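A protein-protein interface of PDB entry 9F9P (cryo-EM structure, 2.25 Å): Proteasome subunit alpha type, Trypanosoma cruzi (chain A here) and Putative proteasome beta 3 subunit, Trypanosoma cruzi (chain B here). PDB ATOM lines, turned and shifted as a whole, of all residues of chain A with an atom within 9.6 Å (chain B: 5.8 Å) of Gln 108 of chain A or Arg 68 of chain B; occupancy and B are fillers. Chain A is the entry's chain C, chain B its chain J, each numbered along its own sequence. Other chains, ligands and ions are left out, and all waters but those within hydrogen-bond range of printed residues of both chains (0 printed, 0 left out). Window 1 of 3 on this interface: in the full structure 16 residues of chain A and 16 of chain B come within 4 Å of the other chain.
The side-chain amino group of Lys 66 of chain B lies within hydrogen-bond range of the side-chain hydroxyl of Tyr 105 of chain A, at 3.1 Å.
The side-chain amide oxygen (OE1) of Gln 108 of chain A sits at hydrogen-bond distance from the guanidinium group (NH2) of Arg 68 of chain B, 3.2 Å away.
The side-chain hydroxyl (OG1) of Thr 106 of chain A lies within hydrogen-bond range of the backbone carbonyl oxygen (O) of Arg 102 of chain A (3.3 Å).
O of His 104 of chain A lies close to NE2 of Gln 108 of chain A, 3.4 Å away.
The backbone carbonyl oxygen of Tyr 105 of chain A lies within hydrogen-bond range of the side-chain amide nitrogen of Gln 108 of chain A.
Among the printed residues, merely in contact across the chains: Asn 101 of chain A with Phe 69 of chain B (3.5 Å), Asn 101 of chain A with Glu 72 of chain B (3.7 Å), Arg 102 of chain A with Phe 69 of chain B (3.8 Å), Tyr 105 of chain A with Glu 65 of chain B (3.8 Å) and Gln 108 of chain A with Glu 65 of chain B (3.6 Å).
Of chain B, only Glu 65 and Arg 68 come within 4 Å of Gln 108 of chain A.
Of the printed residues of chain A, Arg 68 of chain B touches Gln 108.
Glu 65 of chain B touches just these residues of chain A: Tyr 105 (3.8 Å) and Gln 108 (3.6 Å).
Of the printed residues of chain B, Arg 102 of chain A touches Phe 69.
Of the printed residues of chain B, Tyr 105 of chain A touches Glu 65 (3.8 Å) and Lys 66 (3.1 Å).
His 43 of chain B touches none of the printed residues of chain A.
The nearest printed residue of chain B that does not touch Gln 108 of chain A is Gln 61 of chain B (6.9 Å).
The nearest residue of chain A that does not touch Arg 68 of chain B is His 104 of chain A (4.9 Å).
The nearest printed residue of chain B that does not touch Arg 102 of chain A is Leu 73 of chain B (6.6 Å).
Hydrophobic or aromatic side chains of chain B that line the printed part of chain A: Phe 69.
Of the 15 printed residues of chain A, 4 touch a printed residue of chain B.
Printed residues of chain A that touch a printed residue of chain B: Asn 101, Arg 102, Tyr 105 and Gln 108.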
ATOM      1  N   ALA A 100       6.063 -11.968  -2.117  1.00  0.00           N
ATOM      2  CA  ALA A 100       7.401 -12.505  -2.054  1.00  0.00           C
ATOM      3  C   ALA A 100       7.890 -12.877  -3.447  1.00  0.00           C
ATOM      4  O   ALA A 100       9.073 -12.741  -3.713  1.00  0.00           O
ATOM      5  CB  ALA A 100       7.459 -13.703  -1.148  1.00  0.00           C
ATOM      6  N   ASN A 101       7.009 -13.322  -4.328  1.00  0.00           N
ATOM      7  CA  ASN A 101       7.416 -13.687  -5.670  1.00  0.00           C
ATOM      8  C   ASN A 101       7.462 -12.468  -6.591  1.00  0.00           C
ATOM      9  O   ASN A 101       8.140 -12.508  -7.582  1.00  0.00           O
ATOM     10  CB  ASN A 101       6.560 -14.866  -6.182  1.00  0.00           C
ATOM     11  CG  ASN A 101       6.969 -16.203  -5.562  1.00  0.00           C
ATOM     12  OD1 ASN A 101       7.956 -16.797  -6.007  1.00  0.00           O
ATOM     13  ND2 ASN A 101       6.296 -16.653  -4.500  1.00  0.00           N
ATOM     14  N   ARG A 102       6.778 -11.363  -6.316  1.00  0.00           N
ATOM     15  CA  ARG A 102       7.008 -10.158  -7.085  1.00  0.00           C
ATOM     16  C   ARG A 102       8.374  -9.541  -6.812  1.00  0.00           C
ATOM     17  O   ARG A 102       9.008  -9.014  -7.717  1.00  0.00           O
ATOM     18  CB  ARG A 102       6.038  -9.039  -6.766  1.00  0.00           C
ATOM     19  CG  ARG A 102       4.815  -9.024  -7.643  1.00  0.00           C
ATOM     20  CD  ARG A 102       4.142  -7.663  -7.685  1.00  0.00           C
ATOM     21  NE  ARG A 102       2.689  -7.850  -7.585  1.00  0.00           N
ATOM     22  CZ  ARG A 102       2.017  -7.759  -6.441  1.00  0.00           C
ATOM     23  NH1 ARG A 102       2.645  -7.387  -5.336  1.00  0.00           N
ATOM     24  NH2 ARG A 102       0.725  -8.048  -6.399  1.00  0.00           N
ATOM     25  N   HIS A 103       8.784  -9.506  -5.559  1.00  0.00           N
ATOM     26  CA  HIS A 103      10.118  -9.067  -5.239  1.00  0.00           C
ATOM     27  C   HIS A 103      11.151  -9.844  -6.060  1.00  0.00           C
ATOM     28  O   HIS A 103      12.072  -9.283  -6.619  1.00  0.00           O
ATOM     29  CB  HIS A 103      10.342  -9.158  -3.728  1.00  0.00           C
ATOM     30  CG  HIS A 103      11.619  -8.569  -3.246  1.00  0.00           C
ATOM     31  ND1 HIS A 103      12.799  -9.286  -3.377  1.00  0.00           N
ATOM     32  CD2 HIS A 103      11.910  -7.420  -2.581  1.00  0.00           C
ATOM     33  CE1 HIS A 103      13.774  -8.570  -2.806  1.00  0.00           C
ATOM     34  NE2 HIS A 103      13.265  -7.409  -2.336  1.00  0.00           N
ATOM     35  N   HIS A 104      11.022 -11.148  -6.141  1.00  0.00           N
ATOM     36  CA  HIS A 104      11.985 -11.924  -6.886  1.00  0.00           C
ATOM     37  C   HIS A 104      11.932 -11.599  -8.389  1.00  0.00           C
ATOM     38  O   HIS A 104      12.931 -11.597  -9.069  1.00  0.00           O
ATOM     39  CB  HIS A 104      11.767 -13.394  -6.537  1.00  0.00           C
ATOM     40  CG  HIS A 104      12.856 -14.212  -7.115  1.00  0.00           C
ATOM     41  ND1 HIS A 104      12.936 -14.455  -8.469  1.00  0.00           N
ATOM     42  CD2 HIS A 104      13.918 -14.775  -6.550  1.00  0.00           C
ATOM     43  CE1 HIS A 104      14.047 -15.137  -8.702  1.00  0.00           C
ATOM     44  NE2 HIS A 104      14.671 -15.322  -7.550  1.00  0.00           N
ATOM     45  N   TYR A 105      10.768 -11.295  -8.934  1.00  0.00           N
ATOM     46  CA  TYR A 105      10.655 -10.829 -10.294  1.00  0.00           C
ATOM     47  C   TYR A 105      11.414  -9.519 -10.527  1.00  0.00           C
ATOM     48  O   TYR A 105      12.041  -9.345 -11.572  1.00  0.00           O
ATOM     49  CB  TYR A 105       9.183 -10.626 -10.643  1.00  0.00           C
ATOM     50  CG  TYR A 105       8.938  -9.955 -11.968  1.00  0.00           C
ATOM     51  CD1 TYR A 105       9.097 -10.646 -13.160  1.00  0.00           C
ATOM     52  CD2 TYR A 105       8.506  -8.651 -12.035  1.00  0.00           C
ATOM     53  CE1 TYR A 105       8.878 -10.044 -14.388  1.00  0.00           C
ATOM     54  CE2 TYR A 105       8.317  -8.014 -13.256  1.00  0.00           C
ATOM     55  CZ  TYR A 105       8.505  -8.713 -14.439  1.00  0.00           C
ATOM     56  OH  TYR A 105       8.321  -8.101 -15.657  1.00  0.00           O
ATOM     57  N   THR A 106      11.322  -8.566  -9.604  1.00  0.00           N
ATOM     58  CA  THR A 106      11.877  -7.249  -9.811  1.00  0.00           C
ATOM     59  C   THR A 106      13.384  -7.210  -9.570  1.00  0.00           C
ATOM     60  O   THR A 106      14.117  -6.652 -10.365  1.00  0.00           O
ATOM     61  CB  THR A 106      11.182  -6.249  -8.894  1.00  0.00           C
ATOM     62  OG1 THR A 106       9.793  -6.120  -9.177  1.00  0.00           O
ATOM     63  CG2 THR A 106      11.828  -4.889  -9.018  1.00  0.00           C
ATOM     64  N   TYR A 107      13.885  -7.883  -8.531  1.00  0.00           N
ATOM     65  CA  TYR A 107      15.299  -7.832  -8.164  1.00  0.00           C
ATOM     66  C   TYR A 107      16.061  -9.109  -8.461  1.00  0.00           C
ATOM     67  O   TYR A 107      17.257  -9.155  -8.260  1.00  0.00           O
ATOM     68  CB  TYR A 107      15.421  -7.580  -6.666  1.00  0.00           C
ATOM     69  CG  TYR A 107      14.855  -6.248  -6.300  1.00  0.00           C
ATOM     70  CD1 TYR A 107      15.552  -5.073  -6.564  1.00  0.00           C
ATOM     71  CD2 TYR A 107      13.621  -6.141  -5.696  1.00  0.00           C
ATOM     72  CE1 TYR A 107      15.019  -3.835  -6.212  1.00  0.00           C
ATOM     73  CE2 TYR A 107      13.040  -4.912  -5.398  1.00  0.00           C
ATOM     74  CZ  TYR A 107      13.732  -3.748  -5.684  1.00  0.00           C
ATOM     75  OH  TYR A 107      13.163  -2.538  -5.370  1.00  0.00           O
ATOM     76  N   GLN A 108      15.374 -10.170  -8.879  1.00  0.00           N
ATOM     77  CA  GLN A 108      15.990 -11.475  -9.082  1.00  0.00           C
ATOM     78  C   GLN A 108      16.778 -11.922  -7.852  1.00  0.00           C
ATOM     79  O   GLN A 108      17.771 -12.608  -7.976  1.00  0.00           O
ATOM     80  CB  GLN A 108      16.858 -11.469 -10.357  1.00  0.00           C
ATOM     81  CG  GLN A 108      16.085 -11.155 -11.639  1.00  0.00           C
ATOM     82  CD  GLN A 108      15.128 -12.277 -11.960  1.00  0.00           C
ATOM     83  OE1 GLN A 108      15.491 -13.452 -11.871  1.00  0.00           O
ATOM     84  NE2 GLN A 108      13.878 -11.945 -12.278  1.00  0.00           N
ATOM     85  N   GLU A 109      16.358 -11.586  -6.654  1.00  0.00           N
ATOM     86  CA  GLU A 109      16.938 -12.194  -5.466  1.00  0.00           C
ATOM     87  C   GLU A 109      15.804 -12.429  -4.478  1.00  0.00           C
ATOM     88  O   GLU A 109      14.793 -11.775  -4.596  1.00  0.00           O
ATOM     89  CB  GLU A 109      18.021 -11.303  -4.840  1.00  0.00           C
ATOM     90  CG  GLU A 109      17.471 -10.030  -4.229  1.00  0.00           C
ATOM     91  CD  GLU A 109      18.420  -9.218  -3.355  1.00  0.00           C
ATOM     92  OE1 GLU A 109      18.056  -8.031  -3.020  1.00  0.00           O
ATOM     93  OE2 GLU A 109      19.498  -9.768  -2.964  1.00  0.00           O
ATOM     94  N   PRO A 110      15.957 -13.264  -3.422  1.00  0.00           N
ATOM     95  CA  PRO A 110      14.880 -13.473  -2.452  1.00  0.00           C
ATOM     96  C   PRO A 110      14.584 -12.330  -1.491  1.00  0.00           C
ATOM     97  O   PRO A 110      15.483 -11.749  -0.947  1.00  0.00           O
ATOM     98  CB  PRO A 110      15.312 -14.675  -1.607  1.00  0.00           C
ATOM     99  CG  PRO A 110      16.791 -14.876  -1.893  1.00  0.00           C
ATOM    100  CD  PRO A 110      17.181 -13.995  -3.073  1.00  0.00           C
ATOM    101  N   MET A 111      13.304 -12.109  -1.208  1.00  0.00           N
ATOM    102  CA  MET A 111      12.838 -11.170  -0.192  1.00  0.00           C
ATOM    103  C   MET A 111      13.355 -11.513   1.190  1.00  0.00           C
ATOM    104  O   MET A 111      13.280 -12.658   1.613  1.00  0.00           O
ATOM    105  CB  MET A 111      11.313 -11.184  -0.097  1.00  0.00           C
ATOM    106  CG  MET A 111      10.758  -9.940   0.593  1.00  0.00           C
ATOM    107  SD  MET A 111       8.945  -9.793   0.397  1.00  0.00           S
ATOM    108  CE  MET A 111       8.784  -8.058   0.043  1.00  0.00           C
ATOM    109  N   GLU A 234      24.255 -21.077 -17.749  1.00  0.00           N
ATOM    110  CA  GLU A 234      24.421 -19.789 -17.076  1.00  0.00           C
ATOM    111  C   GLU A 234      25.894 -19.515 -16.770  1.00  0.00           C
ATOM    112  O   GLU A 234      26.321 -19.635 -15.629  1.00  0.00           O
ATOM    113  CB  GLU A 234      23.626 -19.707 -15.768  1.00  0.00           C
ATOM    114  CG  GLU A 234      22.141 -19.435 -15.954  1.00  0.00           C
ATOM    115  CD  GLU A 234      21.220 -20.640 -15.835  1.00  0.00           C
ATOM    116  OE1 GLU A 234      21.165 -21.242 -14.730  1.00  0.00           O
ATOM    117  OE2 GLU A 234      20.539 -20.961 -16.841  1.00  0.00           O
ATOM    118  N   VAL A 238      26.254 -17.930 -10.127  1.00  0.00           N
ATOM    119  CA  VAL A 238      27.004 -18.392  -8.966  1.00  0.00           C
ATOM    120  C   VAL A 238      25.998 -18.771  -7.883  1.00  0.00           C
ATOM    121  O   VAL A 238      25.292 -17.898  -7.385  1.00  0.00           O
ATOM    122  CB  VAL A 238      27.991 -17.321  -8.448  1.00  0.00           C
ATOM    123  CG1 VAL A 238      28.877 -17.860  -7.329  1.00  0.00           C
ATOM    124  CG2 VAL A 238      28.852 -16.729  -9.560  1.00  0.00           C
ATOM    125  N   LEU A 239      25.934 -20.069  -7.545  1.00  0.00           N
ATOM    126  CA  LEU A 239      25.220 -20.543  -6.365  1.00  0.00           C
ATOM    127  C   LEU A 239      26.206 -20.694  -5.210  1.00  0.00           C
ATOM    128  O   LEU A 239      27.408 -20.799  -5.445  1.00  0.00           O
ATOM    129  CB  LEU A 239      24.539 -21.886  -6.659  1.00  0.00           C
ATOM    130  CG  LEU A 239      23.250 -21.842  -7.489  1.00  0.00           C
ATOM    131  CD1 LEU A 239      22.628 -23.232  -7.581  1.00  0.00           C
ATOM    132  CD2 LEU A 239      22.239 -20.848  -6.920  1.00  0.00           C
ATOM    133  N   HIS B  43      16.498 -21.987 -21.523  1.00  0.00           N
ATOM    134  CA  HIS B  43      16.025 -21.837 -20.159  1.00  0.00           C
ATOM    135  C   HIS B  43      15.412 -23.151 -19.682  1.00  0.00           C
ATOM    136  O   HIS B  43      14.435 -23.610 -20.248  1.00  0.00           O
ATOM    137  CB  HIS B  43      14.936 -20.758 -20.064  1.00  0.00           C
ATOM    138  CG  HIS B  43      15.311 -19.410 -20.586  1.00  0.00           C
ATOM    139  ND1 HIS B  43      15.750 -18.388 -19.769  1.00  0.00           N
ATOM    140  CD2 HIS B  43      15.340 -18.915 -21.864  1.00  0.00           C
ATOM    141  CE1 HIS B  43      16.062 -17.335 -20.540  1.00  0.00           C
ATOM    142  NE2 HIS B  43      15.794 -17.614 -21.816  1.00  0.00           N
ATOM    143  N   ILE B  45      13.015 -25.109 -17.426  1.00  0.00           N
ATOM    144  CA  ILE B  45      11.794 -24.805 -16.682  1.00  0.00           C
ATOM    145  C   ILE B  45      11.553 -25.807 -15.546  1.00  0.00           C
ATOM    146  O   ILE B  45      11.177 -25.425 -14.453  1.00  0.00           O
ATOM    147  CB  ILE B  45      10.598 -24.747 -17.648  1.00  0.00           C
ATOM    148  CG1 ILE B  45      10.785 -23.672 -18.727  1.00  0.00           C
ATOM    149  CG2 ILE B  45       9.300 -24.551 -16.890  1.00  0.00           C
ATOM    150  CD1 ILE B  45      10.854 -22.225 -18.209  1.00  0.00           C
ATOM    151  N   GLN B  61      14.567 -11.301 -22.346  1.00  0.00           N
ATOM    152  CA  GLN B  61      14.825 -11.259 -20.918  1.00  0.00           C
ATOM    153  C   GLN B  61      13.529 -10.962 -20.162  1.00  0.00           C
ATOM    154  O   GLN B  61      13.263 -11.596 -19.167  1.00  0.00           O
ATOM    155  CB  GLN B  61      15.907 -10.201 -20.601  1.00  0.00           C
ATOM    156  CG  GLN B  61      17.302 -10.554 -21.145  1.00  0.00           C
ATOM    157  CD  GLN B  61      18.376  -9.545 -20.849  1.00  0.00           C
ATOM    158  OE1 GLN B  61      18.449  -8.472 -21.413  1.00  0.00           O
ATOM    159  NE2 GLN B  61      19.261  -9.880 -19.942  1.00  0.00           N
ATOM    160  N   PHE B  63      10.312 -11.472 -21.220  1.00  0.00           N
ATOM    161  CA  PHE B  63       9.323 -12.521 -21.351  1.00  0.00           C
ATOM    162  C   PHE B  63       9.710 -13.764 -20.557  1.00  0.00           C
ATOM    163  O   PHE B  63       8.853 -14.401 -19.954  1.00  0.00           O
ATOM    164  CB  PHE B  63       9.028 -12.794 -22.822  1.00  0.00           C
ATOM    165  CG  PHE B  63       7.942 -13.795 -23.044  1.00  0.00           C
ATOM    166  CD1 PHE B  63       6.622 -13.398 -23.085  1.00  0.00           C
ATOM    167  CD2 PHE B  63       8.246 -15.118 -23.216  1.00  0.00           C
ATOM    168  CE1 PHE B  63       5.613 -14.322 -23.296  1.00  0.00           C
ATOM    169  CE2 PHE B  63       7.248 -16.067 -23.409  1.00  0.00           C
ATOM    170  CZ  PHE B  63       5.938 -15.664 -23.402  1.00  0.00           C
ATOM    171  N   SER B  64      10.978 -14.103 -20.491  1.00  0.00           N
ATOM    172  CA  SER B  64      11.342 -15.254 -19.710  1.00  0.00           C
ATOM    173  C   SER B  64      11.183 -15.007 -18.213  1.00  0.00           C
ATOM    174  O   SER B  64      10.872 -15.925 -17.497  1.00  0.00           O
ATOM    175  CB  SER B  64      12.723 -15.751 -20.034  1.00  0.00           C
ATOM    176  OG  SER B  64      13.721 -14.783 -19.728  1.00  0.00           O
ATOM    177  N   GLU B  65      11.427 -13.804 -17.712  1.00  0.00           N
ATOM    178  CA  GLU B  65      11.141 -13.488 -16.314  1.00  0.00           C
ATOM    179  C   GLU B  65       9.650 -13.593 -15.977  1.00  0.00           C
ATOM    180  O   GLU B  65       9.330 -14.102 -14.926  1.00  0.00           O
ATOM    181  CB  GLU B  65      11.642 -12.087 -15.955  1.00  0.00           C
ATOM    182  CG  GLU B  65      13.155 -12.032 -15.831  1.00  0.00           C
ATOM    183  CD  GLU B  65      13.846 -10.669 -15.941  1.00  0.00           C
ATOM    184  OE1 GLU B  65      13.146  -9.610 -15.851  1.00  0.00           O
ATOM    185  OE2 GLU B  65      15.111 -10.654 -16.140  1.00  0.00           O
ATOM    186  N   LYS B  66       8.748 -13.099 -16.838  1.00  0.00           N
ATOM    187  CA  LYS B  66       7.327 -13.267 -16.611  1.00  0.00           C
ATOM    188  C   LYS B  66       6.911 -14.726 -16.572  1.00  0.00           C
ATOM    189  O   LYS B  66       6.001 -15.071 -15.835  1.00  0.00           O
ATOM    190  CB  LYS B  66       6.462 -12.588 -17.657  1.00  0.00           C
ATOM    191  CG  LYS B  66       6.580 -11.081 -17.648  1.00  0.00           C
ATOM    192  CD  LYS B  66       5.565 -10.383 -18.540  1.00  0.00           C
ATOM    193  CE  LYS B  66       5.862  -8.887 -18.629  1.00  0.00           C
ATOM    194  NZ  LYS B  66       5.723  -8.152 -17.337  1.00  0.00           N
ATOM    195  N   VAL B  67       7.508 -15.567 -17.401  1.00  0.00           N
ATOM    196  CA  VAL B  67       7.174 -16.978 -17.459  1.00  0.00           C
ATOM    197  C   VAL B  67       7.656 -17.690 -16.200  1.00  0.00           C
ATOM    198  O   VAL B  67       6.959 -18.518 -15.685  1.00  0.00           O
ATOM    199  CB  VAL B  67       7.784 -17.604 -18.742  1.00  0.00           C
ATOM    200  CG1 VAL B  67       8.032 -19.096 -18.662  1.00  0.00           C
ATOM    201  CG2 VAL B  67       6.935 -17.317 -19.946  1.00  0.00           C
ATOM    202  N   ARG B  68       8.837 -17.374 -15.711  1.00  0.00           N
ATOM    203  CA  ARG B  68       9.335 -17.944 -14.472  1.00  0.00           C
ATOM    204  C   ARG B  68       8.503 -17.541 -13.241  1.00  0.00           C
ATOM    205  O   ARG B  68       8.340 -18.363 -12.367  1.00  0.00           O
ATOM    206  CB  ARG B  68      10.813 -17.584 -14.281  1.00  0.00           C
ATOM    207  CG  ARG B  68      11.742 -18.381 -15.191  1.00  0.00           C
ATOM    208  CD  ARG B  68      13.194 -18.345 -14.751  1.00  0.00           C
ATOM    209  NE  ARG B  68      13.932 -17.280 -15.422  1.00  0.00           N
ATOM    210  CZ  ARG B  68      14.400 -16.163 -14.856  1.00  0.00           C
ATOM    211  NH1 ARG B  68      14.901 -15.217 -15.634  1.00  0.00           N
ATOM    212  NH2 ARG B  68      14.316 -15.968 -13.546  1.00  0.00           N
ATOM    213  N   PHE B  69       7.991 -16.323 -13.183  1.00  0.00           N
ATOM    214  CA  PHE B  69       7.101 -15.828 -12.137  1.00  0.00           C
ATOM    215  C   PHE B  69       5.768 -16.595 -12.132  1.00  0.00           C
ATOM    216  O   PHE B  69       5.368 -17.068 -11.087  1.00  0.00           O
ATOM    217  CB  PHE B  69       6.929 -14.307 -12.325  1.00  0.00           C
ATOM    218  CG  PHE B  69       5.886 -13.585 -11.505  1.00  0.00           C
ATOM    219  CD1 PHE B  69       4.719 -13.111 -12.094  1.00  0.00           C
ATOM    220  CD2 PHE B  69       6.000 -13.443 -10.137  1.00  0.00           C
ATOM    221  CE1 PHE B  69       3.727 -12.488 -11.339  1.00  0.00           C
ATOM    222  CE2 PHE B  69       5.035 -12.785  -9.387  1.00  0.00           C
ATOM    223  CZ  PHE B  69       3.916 -12.274  -9.986  1.00  0.00           C
ATOM    224  N   ARG B  70       5.110 -16.769 -13.279  1.00  0.00           N
ATOM    225  CA  ARG B  70       3.875 -17.537 -13.355  1.00  0.00           C
ATOM    226  C   ARG B  70       4.079 -18.999 -12.967  1.00  0.00           C
ATOM    227  O   ARG B  70       3.183 -19.598 -12.396  1.00  0.00           O
ATOM    228  CB  ARG B  70       3.264 -17.610 -14.755  1.00  0.00           C
ATOM    229  CG  ARG B  70       2.904 -16.297 -15.417  1.00  0.00           C
ATOM    230  CD  ARG B  70       1.616 -15.705 -14.950  1.00  0.00           C
ATOM    231  NE  ARG B  70       0.957 -15.100 -16.105  1.00  0.00           N
ATOM    232  CZ  ARG B  70      -0.136 -15.592 -16.693  1.00  0.00           C
ATOM    233  NH1 ARG B  70      -0.620 -14.984 -17.766  1.00  0.00           N
ATOM    234  NH2 ARG B  70      -0.729 -16.686 -16.219  1.00  0.00           N
ATOM    235  N   ASN B  71       5.211 -19.570 -13.340  1.00  0.00           N
ATOM    236  CA  ASN B  71       5.518 -20.945 -13.036  1.00  0.00           C
ATOM    237  C   ASN B  71       5.698 -21.121 -11.534  1.00  0.00           C
ATOM    238  O   ASN B  71       5.168 -22.068 -11.023  1.00  0.00           O
ATOM    239  CB  ASN B  71       6.708 -21.446 -13.851  1.00  0.00           C
ATOM    240  CG  ASN B  71       7.133 -22.870 -13.545  1.00  0.00           C
ATOM    241  OD1 ASN B  71       6.376 -23.825 -13.686  1.00  0.00           O
ATOM    242  ND2 ASN B  71       8.381 -23.053 -13.170  1.00  0.00           N
ATOM    243  N   GLU B  72       6.350 -20.184 -10.830  1.00  0.00           N
ATOM    244  CA  GLU B  72       6.494 -20.249  -9.380  1.00  0.00           C
ATOM    245  C   GLU B  72       5.147 -20.202  -8.659  1.00  0.00           C
ATOM    246  O   GLU B  72       4.898 -21.015  -7.793  1.00  0.00           O
ATOM    247  CB  GLU B  72       7.359 -19.134  -8.796  1.00  0.00           C
ATOM    248  CG  GLU B  72       8.879 -19.320  -8.998  1.00  0.00           C
ATOM    249  CD  GLU B  72       9.555 -20.683  -8.727  1.00  0.00           C
ATOM    250  OE1 GLU B  72      10.408 -21.103  -9.570  1.00  0.00           O
ATOM    251  OE2 GLU B  72       9.260 -21.340  -7.679  1.00  0.00           O
ATOM    252  N   LEU B  73       4.257 -19.304  -9.059  1.00  0.00           N
ATOM    253  CA  LEU B  73       2.942 -19.304  -8.465  1.00  0.00           C
ATOM    254  C   LEU B  73       2.113 -20.536  -8.781  1.00  0.00           C
ATOM    255  O   LEU B  73       1.256 -20.869  -7.992  1.00  0.00           O
ATOM    256  CB  LEU B  73       2.146 -18.100  -8.923  1.00  0.00           C
ATOM    257  CG  LEU B  73       2.715 -16.753  -8.515  1.00  0.00           C
ATOM    258  CD1 LEU B  73       1.862 -15.710  -9.188  1.00  0.00           C
ATOM    259  CD2 LEU B  73       2.748 -16.548  -7.004  1.00  0.00           C
